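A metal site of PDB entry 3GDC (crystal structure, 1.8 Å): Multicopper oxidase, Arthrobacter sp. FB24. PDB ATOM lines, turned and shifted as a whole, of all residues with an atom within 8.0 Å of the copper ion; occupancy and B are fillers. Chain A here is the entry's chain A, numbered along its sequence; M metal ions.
N of Ile 111 is in hydrogen-bond range of O of His 88, 2.9 Å away.
The backbone carbonyl oxygen (O) of Leu 146 sits at hydrogen-bond distance from the backbone NH (N) of Cys 133 (3.1 Å).
The backbone NH (N) of Cys 133 is in hydrogen-bond range of the side-chain hydroxyl (OH) of Tyr 59.
The side-chain amide nitrogen of Asn 82 sits close to the backbone NH of His 88 (3.4 Å).
SG of Cys 133 sits close to N of Gln 135, 3.4 Å away.
The backbone NH of Leu 146 lies within hydrogen-bond range of the backbone carbonyl oxygen of Trp 57 (3.2 Å).
The backbone carbonyl oxygen of His 86 lies close to a ring nitrogen (NE2) of His 88 (3.4 Å).
The side-chain sulfur (SG) of Cys 133 lies close to the backbone NH (N) of Thr 89, at 3.4 Å.
The copper ion is bound by ND1 of His 88 (2.1 Å), ND1 of His 141 (2.2 Å) and SG of Cys 133 (2.2 Å).
The copper ion has three donor atoms within binding distance.
Merely in contact with the copper ion: Leu 146 (3.2 Å), Pro 87 (3.7 Å) and Gln 135 (3.7 Å).
The nearest printed residue that does not touch the copper ion is Thr 89 (4.4 Å).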
ATOM      1  N   ALA A  41      28.863   5.336   9.604  1.00  0.00           N
ATOM      2  CA  ALA A  41      29.636   4.245  10.213  1.00  0.00           C
ATOM      3  C   ALA A  41      30.430   3.534   9.121  1.00  0.00           C
ATOM      4  O   ALA A  41      29.881   3.108   8.098  1.00  0.00           O
ATOM      5  CB  ALA A  41      28.735   3.273  11.001  1.00  0.00           C
ATOM      6  N   TRP A  57      35.599  -0.058  13.842  1.00  0.00           N
ATOM      7  CA  TRP A  57      34.309   0.401  13.380  1.00  0.00           C
ATOM      8  C   TRP A  57      34.256   1.857  13.841  1.00  0.00           C
ATOM      9  O   TRP A  57      34.314   2.131  15.037  1.00  0.00           O
ATOM     10  CB  TRP A  57      33.191  -0.377  14.061  1.00  0.00           C
ATOM     11  CG  TRP A  57      33.092  -1.827  13.678  1.00  0.00           C
ATOM     12  CD1 TRP A  57      33.625  -2.436  12.567  1.00  0.00           C
ATOM     13  CD2 TRP A  57      32.393  -2.846  14.392  1.00  0.00           C
ATOM     14  NE1 TRP A  57      33.310  -3.778  12.561  1.00  0.00           N
ATOM     15  CE2 TRP A  57      32.554  -4.052  13.664  1.00  0.00           C
ATOM     16  CE3 TRP A  57      31.663  -2.870  15.591  1.00  0.00           C
ATOM     17  CZ2 TRP A  57      31.997  -5.276  14.095  1.00  0.00           C
ATOM     18  CZ3 TRP A  57      31.106  -4.072  16.005  1.00  0.00           C
ATOM     19  CH2 TRP A  57      31.286  -5.255  15.271  1.00  0.00           C
ATOM     20  N   TYR A  59      32.894   6.117  13.308  1.00  0.00           N
ATOM     21  CA  TYR A  59      32.048   7.167  12.749  1.00  0.00           C
ATOM     22  C   TYR A  59      32.931   8.153  11.991  1.00  0.00           C
ATOM     23  O   TYR A  59      33.836   8.771  12.589  1.00  0.00           O
ATOM     24  CB  TYR A  59      31.311   7.900  13.860  1.00  0.00           C
ATOM     25  CG  TYR A  59      30.323   7.087  14.670  1.00  0.00           C
ATOM     26  CD1 TYR A  59      29.189   6.520  14.070  1.00  0.00           C
ATOM     27  CD2 TYR A  59      30.476   6.947  16.046  1.00  0.00           C
ATOM     28  CE1 TYR A  59      28.267   5.800  14.817  1.00  0.00           C
ATOM     29  CE2 TYR A  59      29.538   6.231  16.809  1.00  0.00           C
ATOM     30  CZ  TYR A  59      28.442   5.661  16.182  1.00  0.00           C
ATOM     31  OH  TYR A  59      27.516   4.963  16.934  1.00  0.00           O
ATOM     32  N   PHE A  80      22.423   9.794   9.993  1.00  0.00           N
ATOM     33  CA  PHE A  80      23.260   8.608  10.137  1.00  0.00           C
ATOM     34  C   PHE A  80      23.109   7.690   8.944  1.00  0.00           C
ATOM     35  O   PHE A  80      21.985   7.379   8.542  1.00  0.00           O
ATOM     36  CB  PHE A  80      22.878   7.864  11.415  1.00  0.00           C
ATOM     37  CG  PHE A  80      23.694   6.611  11.671  1.00  0.00           C
ATOM     38  CD1 PHE A  80      25.089   6.660  11.655  1.00  0.00           C
ATOM     39  CD2 PHE A  80      23.054   5.403  11.946  1.00  0.00           C
ATOM     40  CE1 PHE A  80      25.842   5.498  11.902  1.00  0.00           C
ATOM     41  CE2 PHE A  80      23.798   4.247  12.201  1.00  0.00           C
ATOM     42  CZ  PHE A  80      25.191   4.294  12.171  1.00  0.00           C
ATOM     43  N   ASN A  82      24.720   3.871   7.679  1.00  0.00           N
ATOM     44  CA  ASN A  82      25.552   2.724   8.028  1.00  0.00           C
ATOM     45  C   ASN A  82      26.215   2.185   6.776  1.00  0.00           C
ATOM     46  O   ASN A  82      25.558   1.541   5.945  1.00  0.00           O
ATOM     47  CB  ASN A  82      24.734   1.624   8.740  1.00  0.00           C
ATOM     48  CG  ASN A  82      25.603   0.467   9.193  1.00  0.00           C
ATOM     49  OD1 ASN A  82      26.821   0.488   9.011  1.00  0.00           O
ATOM     50  ND2 ASN A  82      24.988  -0.554   9.788  1.00  0.00           N
ATOM     51  N   HIS A  86      28.080  -4.529   9.469  1.00  0.00           N
ATOM     52  CA  HIS A  86      27.243  -4.978  10.575  1.00  0.00           C
ATOM     53  C   HIS A  86      26.188  -3.926  10.887  1.00  0.00           C
ATOM     54  O   HIS A  86      26.390  -2.742  10.589  1.00  0.00           O
ATOM     55  CB  HIS A  86      28.105  -5.230  11.827  1.00  0.00           C
ATOM     56  CG  HIS A  86      29.264  -6.149  11.585  1.00  0.00           C
ATOM     57  ND1 HIS A  86      30.460  -5.714  11.049  1.00  0.00           N
ATOM     58  CD2 HIS A  86      29.403  -7.473  11.815  1.00  0.00           C
ATOM     59  CE1 HIS A  86      31.289  -6.739  10.960  1.00  0.00           C
ATOM     60  NE2 HIS A  86      30.673  -7.824  11.412  1.00  0.00           N
ATOM     61  N   PRO A  87      25.057  -4.332  11.497  1.00  0.00           N
ATOM     62  CA  PRO A  87      24.082  -3.322  11.918  1.00  0.00           C
ATOM     63  C   PRO A  87      24.685  -2.456  13.017  1.00  0.00           C
ATOM     64  O   PRO A  87      25.489  -2.944  13.817  1.00  0.00           O
ATOM     65  CB  PRO A  87      22.928  -4.149  12.487  1.00  0.00           C
ATOM     66  CG  PRO A  87      23.567  -5.440  12.901  1.00  0.00           C
ATOM     67  CD  PRO A  87      24.596  -5.701  11.831  1.00  0.00           C
ATOM     68  N   HIS A  88      24.294  -1.189  13.052  1.00  0.00           N
ATOM     69  CA  HIS A  88      24.803  -0.243  14.048  1.00  0.00           C
ATOM     70  C   HIS A  88      23.695   0.745  14.404  1.00  0.00           C
ATOM     71  O   HIS A  88      22.656   0.833  13.721  1.00  0.00           O
ATOM     72  CB  HIS A  88      26.016   0.549  13.503  1.00  0.00           C
ATOM     73  CG  HIS A  88      27.221  -0.299  13.203  1.00  0.00           C
ATOM     74  ND1 HIS A  88      27.900  -0.991  14.189  1.00  0.00           N
ATOM     75  CD2 HIS A  88      27.884  -0.545  12.046  1.00  0.00           C
ATOM     76  CE1 HIS A  88      28.910  -1.650  13.635  1.00  0.00           C
ATOM     77  NE2 HIS A  88      28.927  -1.385  12.343  1.00  0.00           N
ATOM     78  N   THR A  89      23.915   1.502  15.477  1.00  0.00           N
ATOM     79  CA  THR A  89      23.028   2.596  15.833  1.00  0.00           C
ATOM     80  C   THR A  89      23.875   3.790  16.313  1.00  0.00           C
ATOM     81  O   THR A  89      25.120   3.697  16.379  1.00  0.00           O
ATOM     82  CB  THR A  89      22.020   2.212  16.976  1.00  0.00           C
ATOM     83  OG1 THR A  89      22.725   2.110  18.205  1.00  0.00           O
ATOM     84  CG2 THR A  89      21.291   0.896  16.688  1.00  0.00           C
ATOM     85  N   ILE A  90      23.214   4.888  16.651  1.00  0.00           N
ATOM     86  CA  ILE A  90      23.821   5.898  17.496  1.00  0.00           C
ATOM     87  C   ILE A  90      22.903   6.123  18.684  1.00  0.00           C
ATOM     88  O   ILE A  90      21.736   6.537  18.527  1.00  0.00           O
ATOM     89  CB  ILE A  90      24.079   7.263  16.817  1.00  0.00           C
ATOM     90  CG1 ILE A  90      24.796   7.112  15.468  1.00  0.00           C
ATOM     91  CG2 ILE A  90      24.873   8.189  17.774  1.00  0.00           C
ATOM     92  CD1 ILE A  90      25.006   8.446  14.713  1.00  0.00           C
ATOM     93  N   ILE A 111      20.106  -0.066  12.691  1.00  0.00           N
ATOM     94  CA  ILE A 111      20.238   0.450  11.332  1.00  0.00           C
ATOM     95  C   ILE A 111      21.086  -0.532  10.537  1.00  0.00           C
ATOM     96  O   ILE A 111      22.258  -0.741  10.849  1.00  0.00           O
ATOM     97  CB  ILE A 111      20.854   1.884  11.284  1.00  0.00           C
ATOM     98  CG1 ILE A 111      20.138   2.856  12.241  1.00  0.00           C
ATOM     99  CG2 ILE A 111      20.918   2.414   9.839  1.00  0.00           C
ATOM    100  CD1 ILE A 111      18.574   2.879  12.164  1.00  0.00           C
ATOM    101  N   HIS A 132      27.380   6.769  21.377  1.00  0.00           N
ATOM    102  CA  HIS A 132      28.042   5.530  20.970  1.00  0.00           C
ATOM    103  C   HIS A 132      27.047   4.547  20.407  1.00  0.00           C
ATOM    104  O   HIS A 132      25.837   4.738  20.540  1.00  0.00           O
ATOM    105  CB  HIS A 132      28.817   4.901  22.157  1.00  0.00           C
ATOM    106  CG  HIS A 132      27.969   4.588  23.349  1.00  0.00           C
ATOM    107  ND1 HIS A 132      27.179   3.470  23.427  1.00  0.00           N
ATOM    108  CD2 HIS A 132      27.812   5.256  24.515  1.00  0.00           C
ATOM    109  CE1 HIS A 132      26.545   3.467  24.595  1.00  0.00           C
ATOM    110  NE2 HIS A 132      26.926   4.535  25.271  1.00  0.00           N
ATOM    111  N   CYS A 133      27.537   3.512  19.741  1.00  0.00           N
ATOM    112  CA  CYS A 133      26.646   2.510  19.186  1.00  0.00           C
ATOM    113  C   CYS A 133      25.989   1.692  20.296  1.00  0.00           C
ATOM    114  O   CYS A 133      26.605   1.451  21.352  1.00  0.00           O
ATOM    115  CB  CYS A 133      27.396   1.603  18.210  1.00  0.00           C
ATOM    116  SG  CYS A 133      26.341   0.326  17.503  1.00  0.00           S
ATOM    117  N   HIS A 134      24.750   1.274  20.081  1.00  0.00           N
ATOM    118  CA  HIS A 134      24.065   0.470  21.092  1.00  0.00           C
ATOM    119  C   HIS A 134      23.580  -0.897  20.560  1.00  0.00           C
ATOM    120  O   HIS A 134      22.680  -1.517  21.134  1.00  0.00           O
ATOM    121  CB  HIS A 134      22.935   1.271  21.740  1.00  0.00           C
ATOM    122  CG  HIS A 134      22.659   0.883  23.161  1.00  0.00           C
ATOM    123  ND1 HIS A 134      22.137  -0.348  23.502  1.00  0.00           N
ATOM    124  CD2 HIS A 134      22.829   1.556  24.323  1.00  0.00           C
ATOM    125  CE1 HIS A 134      22.001  -0.415  24.809  1.00  0.00           C
ATOM    126  NE2 HIS A 134      22.416   0.726  25.335  1.00  0.00           N
ATOM    127  N   GLN A 135      24.172  -1.344  19.465  1.00  0.00           N
ATOM    128  CA  GLN A 135      23.912  -2.673  18.925  1.00  0.00           C
ATOM    129  C   GLN A 135      24.528  -3.764  19.815  1.00  0.00           C
ATOM    130  O   GLN A 135      25.633  -3.587  20.358  1.00  0.00           O
ATOM    131  CB  GLN A 135      24.461  -2.763  17.492  1.00  0.00           C
ATOM    132  CG  GLN A 135      24.198  -4.101  16.753  1.00  0.00           C
ATOM    133  CD  GLN A 135      22.751  -4.265  16.322  1.00  0.00           C
ATOM    134  OE1 GLN A 135      22.273  -5.386  16.104  1.00  0.00           O
ATOM    135  NE2 GLN A 135      22.045  -3.154  16.161  1.00  0.00           N
ATOM    136  N   SER A 136      23.812  -4.871  19.968  1.00  0.00           N
ATOM    137  CA  SER A 136      24.345  -6.041  20.685  1.00  0.00           C
ATOM    138  C   SER A 136      25.108  -6.939  19.720  1.00  0.00           C
ATOM    139  O   SER A 136      24.727  -7.075  18.553  1.00  0.00           O
ATOM    140  CB  SER A 136      23.220  -6.823  21.360  1.00  0.00           C
ATOM    141  OG  SER A 136      22.487  -6.002  22.258  1.00  0.00           O
ATOM    142  N   PRO A 137      26.212  -7.575  20.193  1.00  0.00           N
ATOM    143  CA  PRO A 137      26.810  -7.526  21.526  1.00  0.00           C
ATOM    144  C   PRO A 137      27.433  -6.179  21.833  1.00  0.00           C
ATOM    145  O   PRO A 137      28.246  -5.676  21.034  1.00  0.00           O
ATOM    146  CB  PRO A 137      27.906  -8.603  21.463  1.00  0.00           C
ATOM    147  CG  PRO A 137      28.232  -8.719  20.043  1.00  0.00           C
ATOM    148  CD  PRO A 137      26.960  -8.468  19.294  1.00  0.00           C
ATOM    149  N   LEU A 138      27.065  -5.611  22.983  1.00  0.00           N
ATOM    150  CA  LEU A 138      27.443  -4.254  23.373  1.00  0.00           C
ATOM    151  C   LEU A 138      28.953  -3.986  23.402  1.00  0.00           C
ATOM    152  O   LEU A 138      29.383  -2.929  22.936  1.00  0.00           O
ATOM    153  CB  LEU A 138      26.842  -3.906  24.747  1.00  0.00           C
ATOM    154  CG  LEU A 138      25.557  -3.075  24.895  1.00  0.00           C
ATOM    155  CD1 LEU A 138      25.843  -1.569  24.778  1.00  0.00           C
ATOM    156  CD2 LEU A 138      24.480  -3.518  23.920  1.00  0.00           C
ATOM    157  N   PRO A 140      31.940  -5.206  21.874  1.00  0.00           N
ATOM    158  CA  PRO A 140      32.646  -4.896  20.631  1.00  0.00           C
ATOM    159  C   PRO A 140      32.089  -3.684  19.876  1.00  0.00           C
ATOM    160  O   PRO A 140      32.853  -2.984  19.233  1.00  0.00           O
ATOM    161  CB  PRO A 140      32.482  -6.157  19.782  1.00  0.00           C
ATOM    162  CG  PRO A 140      31.351  -6.899  20.381  1.00  0.00           C
ATOM    163  CD  PRO A 140      31.344  -6.562  21.837  1.00  0.00           C
ATOM    164  N   HIS A 141      30.790  -3.443  19.959  1.00  0.00           N
ATOM    165  CA  HIS A 141      30.200  -2.307  19.232  1.00  0.00           C
ATOM    166  C   HIS A 141      30.659  -0.955  19.756  1.00  0.00           C
ATOM    167  O   HIS A 141      30.810  -0.015  18.984  1.00  0.00           O
ATOM    168  CB  HIS A 141      28.672  -2.437  19.139  1.00  0.00           C
ATOM    169  CG  HIS A 141      28.236  -3.401  18.085  1.00  0.00           C
ATOM    170  ND1 HIS A 141      27.981  -3.029  16.783  1.00  0.00           N
ATOM    171  CD2 HIS A 141      28.050  -4.747  18.133  1.00  0.00           C
ATOM    172  CE1 HIS A 141      27.628  -4.082  16.080  1.00  0.00           C
ATOM    173  NE2 HIS A 141      27.666  -5.143  16.868  1.00  0.00           N
ATOM    174  N   ILE A 142      30.935  -0.864  21.050  1.00  0.00           N
ATOM    175  CA  ILE A 142      31.554   0.350  21.604  1.00  0.00           C
ATOM    176  C   ILE A 142      33.085   0.253  21.442  1.00  0.00           C
ATOM    177  O   ILE A 142      33.726   1.188  20.933  1.00  0.00           O
ATOM    178  CB  ILE A 142      31.167   0.595  23.089  1.00  0.00           C
ATOM    179  CG1 ILE A 142      29.647   0.779  23.224  1.00  0.00           C
ATOM    180  CG2 ILE A 142      31.877   1.840  23.647  1.00  0.00           C
ATOM    181  CD1 ILE A 142      29.148   0.806  24.679  1.00  0.00           C
ATOM    182  N   LYS A 144      35.111  -1.335  19.460  1.00  0.00           N
ATOM    183  CA  LYS A 144      35.682  -1.258  18.120  1.00  0.00           C
ATOM    184  C   LYS A 144      35.823   0.160  17.581  1.00  0.00           C
ATOM    185  O   LYS A 144      36.459   0.367  16.553  1.00  0.00           O
ATOM    186  CB  LYS A 144      34.942  -2.177  17.125  1.00  0.00           C
ATOM    187  CG  LYS A 144      35.054  -3.663  17.457  1.00  0.00           C
ATOM    188  CD  LYS A 144      36.140  -4.355  16.659  1.00  0.00           C
ATOM    189  CE  LYS A 144      35.681  -4.662  15.243  1.00  0.00           C
ATOM    190  NZ  LYS A 144      36.754  -5.350  14.476  1.00  0.00           N
ATOM    191  N   LEU A 146      33.133   2.900  17.931  1.00  0.00           N
ATOM    192  CA  LEU A 146      31.909   3.684  17.688  1.00  0.00           C
ATOM    193  C   LEU A 146      31.482   4.532  18.892  1.00  0.00           C
ATOM    194  O   LEU A 146      30.574   4.179  19.644  1.00  0.00           O
ATOM    195  CB  LEU A 146      30.762   2.778  17.201  1.00  0.00           C
ATOM    196  CG  LEU A 146      30.989   2.109  15.846  1.00  0.00           C
ATOM    197  CD1 LEU A 146      29.896   1.080  15.597  1.00  0.00           C
ATOM    198  CD2 LEU A 146      31.063   3.118  14.696  1.00  0.00           C
HETATM  199 CU    CU M   1      27.505  -0.999  16.208  1.00  0.00          CU
